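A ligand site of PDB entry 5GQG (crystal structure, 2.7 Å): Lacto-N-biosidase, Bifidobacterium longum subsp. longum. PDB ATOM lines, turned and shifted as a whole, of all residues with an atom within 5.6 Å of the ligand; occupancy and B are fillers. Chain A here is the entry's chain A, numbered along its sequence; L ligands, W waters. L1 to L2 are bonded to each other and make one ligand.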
ATOM      1  N   VAL A 118      11.383 -27.174 -26.383  1.00  0.00           N
ATOM      2  CA  VAL A 118      12.131 -27.386 -25.144  1.00  0.00           C
ATOM      3  C   VAL A 118      12.348 -26.084 -24.358  1.00  0.00           C
ATOM      4  O   VAL A 118      13.289 -25.998 -23.587  1.00  0.00           O
ATOM      5  CB  VAL A 118      13.470 -28.114 -25.401  1.00  0.00           C
ATOM      6  CG1 VAL A 118      13.214 -29.518 -25.953  1.00  0.00           C
ATOM      7  CG2 VAL A 118      14.336 -27.345 -26.367  1.00  0.00           C
ATOM      8  N   GLY A 119      11.445 -25.113 -24.543  1.00  0.00           N
ATOM      9  CA  GLY A 119      11.507 -23.809 -23.851  1.00  0.00           C
ATOM     10  C   GLY A 119      11.795 -22.674 -24.809  1.00  0.00           C
ATOM     11  O   GLY A 119      11.888 -22.916 -26.008  1.00  0.00           O
ATOM     12  N   ASN A 120      11.916 -21.446 -24.289  1.00  0.00           N
ATOM     13  CA  ASN A 120      12.264 -20.305 -25.159  1.00  0.00           C
ATOM     14  C   ASN A 120      13.746 -20.313 -25.437  1.00  0.00           C
ATOM     15  O   ASN A 120      14.546 -19.647 -24.762  1.00  0.00           O
ATOM     16  CB  ASN A 120      11.859 -18.971 -24.550  1.00  0.00           C
ATOM     17  CG  ASN A 120      10.363 -18.792 -24.481  1.00  0.00           C
ATOM     18  OD1 ASN A 120       9.586 -19.633 -24.951  1.00  0.00           O
ATOM     19  ND2 ASN A 120       9.938 -17.701 -23.858  1.00  0.00           N
ATOM     20  N   HIS A 121      14.107 -21.095 -26.448  1.00  0.00           N
ATOM     21  CA  HIS A 121      15.476 -21.300 -26.818  1.00  0.00           C
ATOM     22  C   HIS A 121      15.536 -21.812 -28.242  1.00  0.00           C
ATOM     23  O   HIS A 121      14.621 -22.562 -28.660  1.00  0.00           O
ATOM     24  CB  HIS A 121      16.093 -22.387 -25.941  1.00  0.00           C
ATOM     25  CG  HIS A 121      16.088 -22.068 -24.472  1.00  0.00           C
ATOM     26  ND1 HIS A 121      16.871 -21.065 -23.924  1.00  0.00           N
ATOM     27  CD2 HIS A 121      15.413 -22.628 -23.441  1.00  0.00           C
ATOM     28  CE1 HIS A 121      16.672 -21.025 -22.628  1.00  0.00           C
ATOM     29  NE2 HIS A 121      15.812 -21.974 -22.297  1.00  0.00           N
ATOM     30  N   LYS A 215      21.538 -21.419 -25.053  1.00  0.00           N
ATOM     31  CA  LYS A 215      21.711 -22.340 -23.933  1.00  0.00           C
ATOM     32  C   LYS A 215      21.542 -23.817 -24.271  1.00  0.00           C
ATOM     33  O   LYS A 215      22.074 -24.680 -23.551  1.00  0.00           O
ATOM     34  CB  LYS A 215      20.765 -21.960 -22.794  1.00  0.00           C
ATOM     35  CG  LYS A 215      21.261 -20.784 -21.966  1.00  0.00           C
ATOM     36  CD  LYS A 215      20.188 -20.356 -20.979  1.00  0.00           C
ATOM     37  CE  LYS A 215      20.411 -20.952 -19.604  1.00  0.00           C
ATOM     38  NZ  LYS A 215      19.105 -21.126 -18.954  1.00  0.00           N
ATOM     39  N   HIS A 216      20.786 -24.140 -25.321  1.00  0.00           N
ATOM     40  CA  HIS A 216      20.530 -25.571 -25.560  1.00  0.00           C
ATOM     41  C   HIS A 216      20.779 -26.098 -26.932  1.00  0.00           C
ATOM     42  O   HIS A 216      20.324 -27.187 -27.257  1.00  0.00           O
ATOM     43  CB  HIS A 216      19.153 -25.928 -25.048  1.00  0.00           C
ATOM     44  CG  HIS A 216      18.998 -25.652 -23.594  1.00  0.00           C
ATOM     45  ND1 HIS A 216      19.763 -26.298 -22.640  1.00  0.00           N
ATOM     46  CD2 HIS A 216      18.242 -24.749 -22.924  1.00  0.00           C
ATOM     47  CE1 HIS A 216      19.455 -25.830 -21.450  1.00  0.00           C
ATOM     48  NE2 HIS A 216      18.535 -24.889 -21.592  1.00  0.00           N
ATOM     49  N   TRP A 264      28.228 -22.847 -23.118  1.00  0.00           N
ATOM     50  CA  TRP A 264      28.387 -23.717 -21.929  1.00  0.00           C
ATOM     51  C   TRP A 264      29.794 -24.322 -21.853  1.00  0.00           C
ATOM     52  O   TRP A 264      30.409 -24.598 -22.877  1.00  0.00           O
ATOM     53  CB  TRP A 264      27.365 -24.872 -21.872  1.00  0.00           C
ATOM     54  CG  TRP A 264      26.679 -24.993 -20.551  1.00  0.00           C
ATOM     55  CD1 TRP A 264      27.216 -25.366 -19.361  1.00  0.00           C
ATOM     56  CD2 TRP A 264      25.324 -24.665 -20.291  1.00  0.00           C
ATOM     57  NE1 TRP A 264      26.276 -25.288 -18.364  1.00  0.00           N
ATOM     58  CE2 TRP A 264      25.106 -24.853 -18.918  1.00  0.00           C
ATOM     59  CE3 TRP A 264      24.269 -24.218 -21.083  1.00  0.00           C
ATOM     60  CZ2 TRP A 264      23.869 -24.601 -18.308  1.00  0.00           C
ATOM     61  CZ3 TRP A 264      23.027 -23.972 -20.478  1.00  0.00           C
ATOM     62  CH2 TRP A 264      22.845 -24.165 -19.100  1.00  0.00           C
ATOM     63  N   TYR A 270      20.079 -32.382 -21.148  1.00  0.00           N
ATOM     64  CA  TYR A 270      18.922 -31.645 -21.667  1.00  0.00           C
ATOM     65  C   TYR A 270      18.289 -32.546 -22.708  1.00  0.00           C
ATOM     66  O   TYR A 270      18.991 -33.048 -23.615  1.00  0.00           O
ATOM     67  CB  TYR A 270      19.325 -30.273 -22.256  1.00  0.00           C
ATOM     68  CG  TYR A 270      18.221 -29.249 -22.216  1.00  0.00           C
ATOM     69  CD1 TYR A 270      17.819 -28.684 -21.014  1.00  0.00           C
ATOM     70  CD2 TYR A 270      17.571 -28.831 -23.381  1.00  0.00           C
ATOM     71  CE1 TYR A 270      16.793 -27.720 -20.956  1.00  0.00           C
ATOM     72  CE2 TYR A 270      16.541 -27.878 -23.345  1.00  0.00           C
ATOM     73  CZ  TYR A 270      16.154 -27.317 -22.134  1.00  0.00           C
ATOM     74  OH  TYR A 270      15.161 -26.375 -22.085  1.00  0.00           O
ATOM     75  N   ASP A 312      27.823 -20.728 -18.320  1.00  0.00           N
ATOM     76  CA  ASP A 312      27.838 -21.535 -17.114  1.00  0.00           C
ATOM     77  C   ASP A 312      29.020 -22.503 -17.221  1.00  0.00           C
ATOM     78  O   ASP A 312      29.435 -22.810 -18.347  1.00  0.00           O
ATOM     79  CB  ASP A 312      26.527 -22.297 -16.986  1.00  0.00           C
ATOM     80  CG  ASP A 312      25.301 -21.408 -17.156  1.00  0.00           C
ATOM     81  OD1 ASP A 312      24.872 -21.136 -18.351  1.00  0.00           O
ATOM     82  OD2 ASP A 312      24.774 -21.009 -16.096  1.00  0.00           O
ATOM     83  N   THR A 315      26.874 -28.164 -15.801  1.00  0.00           N
ATOM     84  CA  THR A 315      25.470 -28.325 -15.476  1.00  0.00           C
ATOM     85  C   THR A 315      24.952 -29.730 -15.801  1.00  0.00           C
ATOM     86  O   THR A 315      25.297 -30.338 -16.812  1.00  0.00           O
ATOM     87  CB  THR A 315      24.606 -27.268 -16.189  1.00  0.00           C
ATOM     88  OG1 THR A 315      25.167 -25.977 -15.961  1.00  0.00           O
ATOM     89  CG2 THR A 315      23.175 -27.250 -15.626  1.00  0.00           C
ATOM     90  N   MET A 317      21.474 -31.748 -16.295  1.00  0.00           N
ATOM     91  CA  MET A 317      20.105 -31.471 -16.641  1.00  0.00           C
ATOM     92  C   MET A 317      19.363 -32.785 -16.748  1.00  0.00           C
ATOM     93  O   MET A 317      19.871 -33.723 -17.349  1.00  0.00           O
ATOM     94  CB  MET A 317      20.031 -30.767 -17.987  1.00  0.00           C
ATOM     95  CG  MET A 317      20.654 -29.389 -17.980  1.00  0.00           C
ATOM     96  SD  MET A 317      21.312 -28.975 -19.604  1.00  0.00           S
ATOM     97  CE  MET A 317      22.201 -27.444 -19.264  1.00  0.00           C
ATOM     98  N   TYR A 318      18.177 -32.833 -16.167  1.00  0.00           N
ATOM     99  CA  TYR A 318      17.320 -33.983 -16.270  1.00  0.00           C
ATOM    100  C   TYR A 318      18.063 -35.282 -15.954  1.00  0.00           C
ATOM    101  O   TYR A 318      17.956 -36.263 -16.676  1.00  0.00           O
ATOM    102  CB  TYR A 318      16.644 -33.978 -17.634  1.00  0.00           C
ATOM    103  CG  TYR A 318      15.768 -32.765 -17.795  1.00  0.00           C
ATOM    104  CD1 TYR A 318      14.560 -32.688 -17.136  1.00  0.00           C
ATOM    105  CD2 TYR A 318      16.176 -31.683 -18.565  1.00  0.00           C
ATOM    106  CE1 TYR A 318      13.757 -31.558 -17.245  1.00  0.00           C
ATOM    107  CE2 TYR A 318      15.388 -30.548 -18.698  1.00  0.00           C
ATOM    108  CZ  TYR A 318      14.175 -30.483 -18.036  1.00  0.00           C
ATOM    109  OH  TYR A 318      13.386 -29.350 -18.144  1.00  0.00           O
ATOM    110  N   VAL A 351      22.583 -14.531 -17.864  1.00  0.00           N
ATOM    111  CA  VAL A 351      22.432 -15.120 -16.564  1.00  0.00           C
ATOM    112  C   VAL A 351      23.270 -16.437 -16.546  1.00  0.00           C
ATOM    113  O   VAL A 351      23.156 -17.282 -17.455  1.00  0.00           O
ATOM    114  CB  VAL A 351      20.898 -15.213 -16.270  1.00  0.00           C
ATOM    115  CG1 VAL A 351      20.374 -16.627 -16.215  1.00  0.00           C
ATOM    116  CG2 VAL A 351      20.570 -14.465 -14.994  1.00  0.00           C
ATOM    117  N   ALA A 352      24.154 -16.562 -15.550  1.00  0.00           N
ATOM    118  CA  ALA A 352      24.893 -17.782 -15.364  1.00  0.00           C
ATOM    119  C   ALA A 352      25.400 -18.024 -13.948  1.00  0.00           C
ATOM    120  O   ALA A 352      25.866 -17.123 -13.260  1.00  0.00           O
ATOM    121  CB  ALA A 352      26.057 -17.831 -16.329  1.00  0.00           C
ATOM    122  N   ALA A 353      25.348 -19.305 -13.564  1.00  0.00           N
ATOM    123  CA  ALA A 353      25.947 -19.838 -12.344  1.00  0.00           C
ATOM    124  C   ALA A 353      27.053 -20.848 -12.681  1.00  0.00           C
ATOM    125  O   ALA A 353      27.173 -21.288 -13.837  1.00  0.00           O
ATOM    126  CB  ALA A 353      24.880 -20.516 -11.524  1.00  0.00           C
ATOM    127  N   TRP A 356      26.205 -26.617 -11.093  1.00  0.00           N
ATOM    128  CA  TRP A 356      24.815 -26.739 -10.609  1.00  0.00           C
ATOM    129  C   TRP A 356      23.939 -27.740 -11.388  1.00  0.00           C
ATOM    130  O   TRP A 356      24.311 -28.117 -12.488  1.00  0.00           O
ATOM    131  CB  TRP A 356      24.113 -25.360 -10.582  1.00  0.00           C
ATOM    132  CG  TRP A 356      24.051 -24.675 -11.958  1.00  0.00           C
ATOM    133  CD1 TRP A 356      25.071 -24.106 -12.627  1.00  0.00           C
ATOM    134  CD2 TRP A 356      22.881 -24.494 -12.781  1.00  0.00           C
ATOM    135  NE1 TRP A 356      24.637 -23.575 -13.807  1.00  0.00           N
ATOM    136  CE2 TRP A 356      23.296 -23.810 -13.936  1.00  0.00           C
ATOM    137  CE3 TRP A 356      21.529 -24.832 -12.643  1.00  0.00           C
ATOM    138  CZ2 TRP A 356      22.403 -23.466 -14.961  1.00  0.00           C
ATOM    139  CZ3 TRP A 356      20.653 -24.504 -13.644  1.00  0.00           C
ATOM    140  CH2 TRP A 356      21.087 -23.810 -14.794  1.00  0.00           C
ATOM    141  N   TRP A 358      19.898 -28.951 -12.926  1.00  0.00           N
ATOM    142  CA  TRP A 358      18.614 -28.438 -13.416  1.00  0.00           C
ATOM    143  C   TRP A 358      17.644 -29.599 -13.539  1.00  0.00           C
ATOM    144  O   TRP A 358      17.931 -30.567 -14.238  1.00  0.00           O
ATOM    145  CB  TRP A 358      18.762 -27.722 -14.769  1.00  0.00           C
ATOM    146  CG  TRP A 358      17.424 -27.497 -15.457  1.00  0.00           C
ATOM    147  CD1 TRP A 358      16.892 -28.230 -16.479  1.00  0.00           C
ATOM    148  CD2 TRP A 358      16.446 -26.505 -15.138  1.00  0.00           C
ATOM    149  NE1 TRP A 358      15.671 -27.730 -16.833  1.00  0.00           N
ATOM    150  CE2 TRP A 358      15.375 -26.672 -16.021  1.00  0.00           C
ATOM    151  CE3 TRP A 358      16.400 -25.454 -14.210  1.00  0.00           C
ATOM    152  CZ2 TRP A 358      14.238 -25.867 -15.986  1.00  0.00           C
ATOM    153  CZ3 TRP A 358      15.281 -24.663 -14.176  1.00  0.00           C
ATOM    154  CH2 TRP A 358      14.198 -24.879 -15.059  1.00  0.00           C
ATOM    155  N   ASP A 382      22.823 -13.430 -12.151  1.00  0.00           N
ATOM    156  CA  ASP A 382      23.167 -14.444 -11.205  1.00  0.00           C
ATOM    157  C   ASP A 382      24.606 -14.150 -10.771  1.00  0.00           C
ATOM    158  O   ASP A 382      24.874 -13.030 -10.268  1.00  0.00           O
ATOM    159  CB  ASP A 382      22.966 -15.840 -11.874  1.00  0.00           C
ATOM    160  CG  ASP A 382      21.475 -16.264 -11.955  1.00  0.00           C
ATOM    161  OD1 ASP A 382      20.702 -16.084 -10.987  1.00  0.00           O
ATOM    162  OD2 ASP A 382      21.101 -16.819 -12.997  1.00  0.00           O
ATOM    163  N   GLN A 384      26.594 -16.804  -9.025  1.00  0.00           N
ATOM    164  CA  GLN A 384      26.873 -17.652  -7.860  1.00  0.00           C
ATOM    165  C   GLN A 384      27.808 -18.804  -8.212  1.00  0.00           C
ATOM    166  O   GLN A 384      27.866 -19.229  -9.360  1.00  0.00           O
ATOM    167  CB  GLN A 384      25.589 -18.283  -7.296  1.00  0.00           C
ATOM    168  CG  GLN A 384      24.382 -17.359  -7.053  1.00  0.00           C
ATOM    169  CD  GLN A 384      23.526 -17.119  -8.269  1.00  0.00           C
ATOM    170  OE1 GLN A 384      23.964 -17.398  -9.376  1.00  0.00           O
ATOM    171  NE2 GLN A 384      22.315 -16.600  -8.093  1.00  0.00           N
ATOM    172  N   ASP A 387      24.086 -23.392  -7.489  1.00  0.00           N
ATOM    173  CA  ASP A 387      22.690 -23.035  -7.793  1.00  0.00           C
ATOM    174  C   ASP A 387      21.809 -24.273  -7.718  1.00  0.00           C
ATOM    175  O   ASP A 387      21.607 -24.965  -8.724  1.00  0.00           O
ATOM    176  CB  ASP A 387      22.592 -22.380  -9.188  1.00  0.00           C
ATOM    177  CG  ASP A 387      21.154 -22.227  -9.676  1.00  0.00           C
ATOM    178  OD1 ASP A 387      20.186 -22.219  -8.885  1.00  0.00           O
ATOM    179  OD2 ASP A 387      20.992 -22.148 -10.907  1.00  0.00           O
ATOM    180  N   ASP A 389      18.977 -25.069  -8.450  1.00  0.00           N
ATOM    181  CA  ASP A 389      17.928 -24.539  -9.305  1.00  0.00           C
ATOM    182  C   ASP A 389      16.699 -25.439  -9.222  1.00  0.00           C
ATOM    183  O   ASP A 389      16.639 -26.305  -8.350  1.00  0.00           O
ATOM    184  CB  ASP A 389      18.437 -24.443 -10.739  1.00  0.00           C
ATOM    185  CG  ASP A 389      17.855 -23.278 -11.454  1.00  0.00           C
ATOM    186  OD1 ASP A 389      16.632 -23.282 -11.632  1.00  0.00           O
ATOM    187  OD2 ASP A 389      18.617 -22.349 -11.788  1.00  0.00           O
ATOM    188  N   TYR A 390      15.718 -25.248 -10.113  1.00  0.00           N
ATOM    189  CA  TYR A 390      14.557 -26.164 -10.194  1.00  0.00           C
ATOM    190  C   TYR A 390      14.987 -27.615 -10.114  1.00  0.00           C
ATOM    191  O   TYR A 390      16.057 -27.991 -10.581  1.00  0.00           O
ATOM    192  CB  TYR A 390      13.764 -25.969 -11.481  1.00  0.00           C
ATOM    193  CG  TYR A 390      12.790 -24.831 -11.483  1.00  0.00           C
ATOM    194  CD1 TYR A 390      12.896 -23.781 -10.563  1.00  0.00           C
ATOM    195  CD2 TYR A 390      11.746 -24.789 -12.382  1.00  0.00           C
ATOM    196  CE1 TYR A 390      12.003 -22.719 -10.573  1.00  0.00           C
ATOM    197  CE2 TYR A 390      10.847 -23.727 -12.405  1.00  0.00           C
ATOM    198  CZ  TYR A 390      10.984 -22.688 -11.485  1.00  0.00           C
ATOM    199  OH  TYR A 390      10.117 -21.618 -11.452  1.00  0.00           O
ATOM    200  N   MET A 410      22.740 -20.126  -4.625  1.00  0.00           N
ATOM    201  CA  MET A 410      21.357 -19.743  -4.832  1.00  0.00           C
ATOM    202  C   MET A 410      20.474 -20.957  -4.686  1.00  0.00           C
ATOM    203  O   MET A 410      20.885 -22.081  -4.947  1.00  0.00           O
ATOM    204  CB  MET A 410      21.166 -19.162  -6.223  1.00  0.00           C
ATOM    205  CG  MET A 410      19.736 -18.765  -6.606  1.00  0.00           C
ATOM    206  SD  MET A 410      19.750 -18.293  -8.357  1.00  0.00           S
ATOM    207  CE  MET A 410      18.226 -17.383  -8.418  1.00  0.00           C
ATOM    208  N   CYS A 412      16.792 -21.479  -6.221  1.00  0.00           N
ATOM    209  CA  CYS A 412      16.162 -20.641  -7.232  1.00  0.00           C
ATOM    210  C   CYS A 412      14.696 -20.885  -7.455  1.00  0.00           C
ATOM    211  O   CYS A 412      14.316 -21.867  -8.065  1.00  0.00           O
ATOM    212  CB  CYS A 412      16.887 -20.802  -8.552  1.00  0.00           C
ATOM    213  SG  CYS A 412      16.260 -19.608  -9.741  1.00  0.00           S
ATOM    214  N   ASN A 413      13.863 -19.953  -7.010  1.00  0.00           N
ATOM    215  CA  ASN A 413      12.423 -19.894  -7.340  1.00  0.00           C
ATOM    216  C   ASN A 413      11.588 -21.093  -6.827  1.00  0.00           C
ATOM    217  O   ASN A 413      12.111 -21.999  -6.205  1.00  0.00           O
ATOM    218  CB  ASN A 413      12.203 -19.689  -8.875  1.00  0.00           C
ATOM    219  CG  ASN A 413      12.482 -18.263  -9.352  1.00  0.00           C
ATOM    220  OD1 ASN A 413      13.056 -17.429  -8.654  1.00  0.00           O
ATOM    221  ND2 ASN A 413      12.077 -17.994 -10.591  1.00  0.00           N
HETATM  222  C1  LIG L   1      18.406 -19.223 -12.718  1.00  0.00           C
HETATM  223  C2  LIG L   1      17.458 -19.765 -13.776  1.00  0.00           C
HETATM  224  C3  LIG L   1      18.023 -20.831 -14.746  1.00  0.00           C
HETATM  225  C4  LIG L   1      19.474 -20.582 -15.084  1.00  0.00           C
HETATM  226  C5  LIG L   1      20.264 -20.326 -13.809  1.00  0.00           C
HETATM  227  C6  LIG L   1      21.765 -20.190 -14.064  1.00  0.00           C
HETATM  228  C7  LIG L   1      15.006 -19.850 -13.382  1.00  0.00           C
HETATM  229  C8  LIG L   1      13.968 -20.564 -12.568  1.00  0.00           C
HETATM  230  N1  LIG L   1      16.266 -20.242 -13.100  1.00  0.00           N
HETATM  231  O1  LIG L   1      17.935 -17.904 -12.370  1.00  0.00           O
HETATM  232  O2  LIG L   1      17.283 -20.789 -15.982  1.00  0.00           O
HETATM  233  O3  LIG L   1      19.578 -19.453 -15.944  1.00  0.00           O
HETATM  234  O4  LIG L   1      19.755 -19.146 -13.194  1.00  0.00           O
HETATM  235  O5  LIG L   1      22.084 -18.842 -14.415  1.00  0.00           O
HETATM  236  O6  LIG L   1      14.680 -19.011 -14.225  1.00  0.00           O
HETATM  237  C1  LG2 L   2      16.787 -22.011 -16.576  1.00  0.00           C
HETATM  238  C2  LG2 L   2      15.788 -21.633 -17.650  1.00  0.00           C
HETATM  239  C3  LG2 L   2      15.336 -22.893 -18.409  1.00  0.00           C
HETATM  240  C4  LG2 L   2      16.555 -23.616 -18.956  1.00  0.00           C
HETATM  241  C5  LG2 L   2      17.455 -23.951 -17.783  1.00  0.00           C
HETATM  242  C6  LG2 L   2      18.753 -24.640 -18.133  1.00  0.00           C
HETATM  243  O1  LG2 L   2      14.768 -20.889 -16.969  1.00  0.00           O
HETATM  244  O2  LG2 L   2      14.506 -22.624 -19.528  1.00  0.00           O
HETATM  245  O3  LG2 L   2      17.241 -22.787 -19.901  1.00  0.00           O
HETATM  246  O4  LG2 L   2      17.846 -22.752 -17.181  1.00  0.00           O
HETATM  247  O5  LG2 L   2      18.511 -26.049 -18.292  1.00  0.00           O
HETATM  248  O   HOH W   1      16.265 -18.278 -16.281  1.00  0.00           O
HETATM  249  O   HOH W   2      22.289 -19.966 -17.408  1.00  0.00           O
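A ring nitrogen (NE2) of His 216 lies within hydrogen-bond range of an oxygen (O3) of LG2 L2. A ring nitrogen (NE2) of His 121 lies within hydrogen-bond range of an oxygen (O3) of LG2 L2 (2.9 Å). The side-chain sulfur (SG) of Cys 412 is in hydrogen-bond range of a nitrogen (N1) of LIG L1 (3.4 Å). OD1 of Asp 389 sits at hydrogen-bond distance from N1 of LIG L1 (3.4 Å). The backbone NH of Ala 353 sits at hydrogen-bond distance from an oxygen (O5) of LIG L1 (3.4 Å). O5 of LIG L1 sits at hydrogen-bond distance from OD2 of Asp 382 (2.7 Å). The side-chain amino group (NZ) of Lys 215 sits at hydrogen-bond distance from an oxygen (O3) of LG2 L2 (2.7 Å). N of Ala 352 lies close to O5 of LIG L1, at 3.3 Å.
The backbone NH of Asp 389 sits close to the side-chain carboxylate of Asp 387, at 3.1 Å. The side-chain hydroxyl (OG1) of Thr 315 lies within hydrogen-bond range of the indole nitrogen (NE1) of Trp 356 (3.3 Å). The backbone carbonyl oxygen (O) of Ala 353 is in hydrogen-bond range of the indole nitrogen (NE1) of Trp 356 (3.4 Å). N of Ala 353 sits at hydrogen-bond distance from OD2 of Asp 312, 3.1 Å away. The side-chain hydroxyl (OH) of Tyr 270 is in hydrogen-bond range of the backbone carbonyl oxygen (O) of Val 118, 2.4 Å away. NE1 of Trp 356 sits at hydrogen-bond distance from OD2 of Asp 312 (3.4 Å). SD of Met 410 lies within hydrogen-bond range of NE2 of Gln 384. OD1 of Asp 382 sits at hydrogen-bond distance from NE2 of Gln 384.
Merely in contact with the ligand: Val 351 (2.9 Å), Trp 358 (3.3 Å), Trp 356 (3.5 Å), Asp 387 (3.5 Å), Tyr 390 (3.5 Å), Tyr 270 (3.6 Å), Asp 312 (3.7 Å), Asn 413 (3.8 Å), Met 317 (3.98 Å) and Met 410 (3.997 Å). Hydrophobic or aromatic side chains within 4 Å of the ligand: His 121, His 216, Tyr 270, Met 317, Val 351, Trp 356, Trp 358, Tyr 390 and Met 410. Within 4 Å of the ligand: His 121, Lys 215, His 216, Tyr 270, Asp 312, Met 317, Val 351, Ala 352, Ala 353, Trp 356, Trp 358, Asp 382, Asp 387, Asp 389, Tyr 390, Met 410, Cys 412 and Asn 413. The nearest printed residue that does not touch the ligand is Trp 264 (4.2 Å).
Water W2 lies within hydrogen-bond range of the backbone carbonyl oxygen (O) of Val 351 (2.8 Å), the side-chain carboxylate (OD1) of Asp 312 (3.0 Å) and an oxygen (O3) of LIG L1 (3.1 Å).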
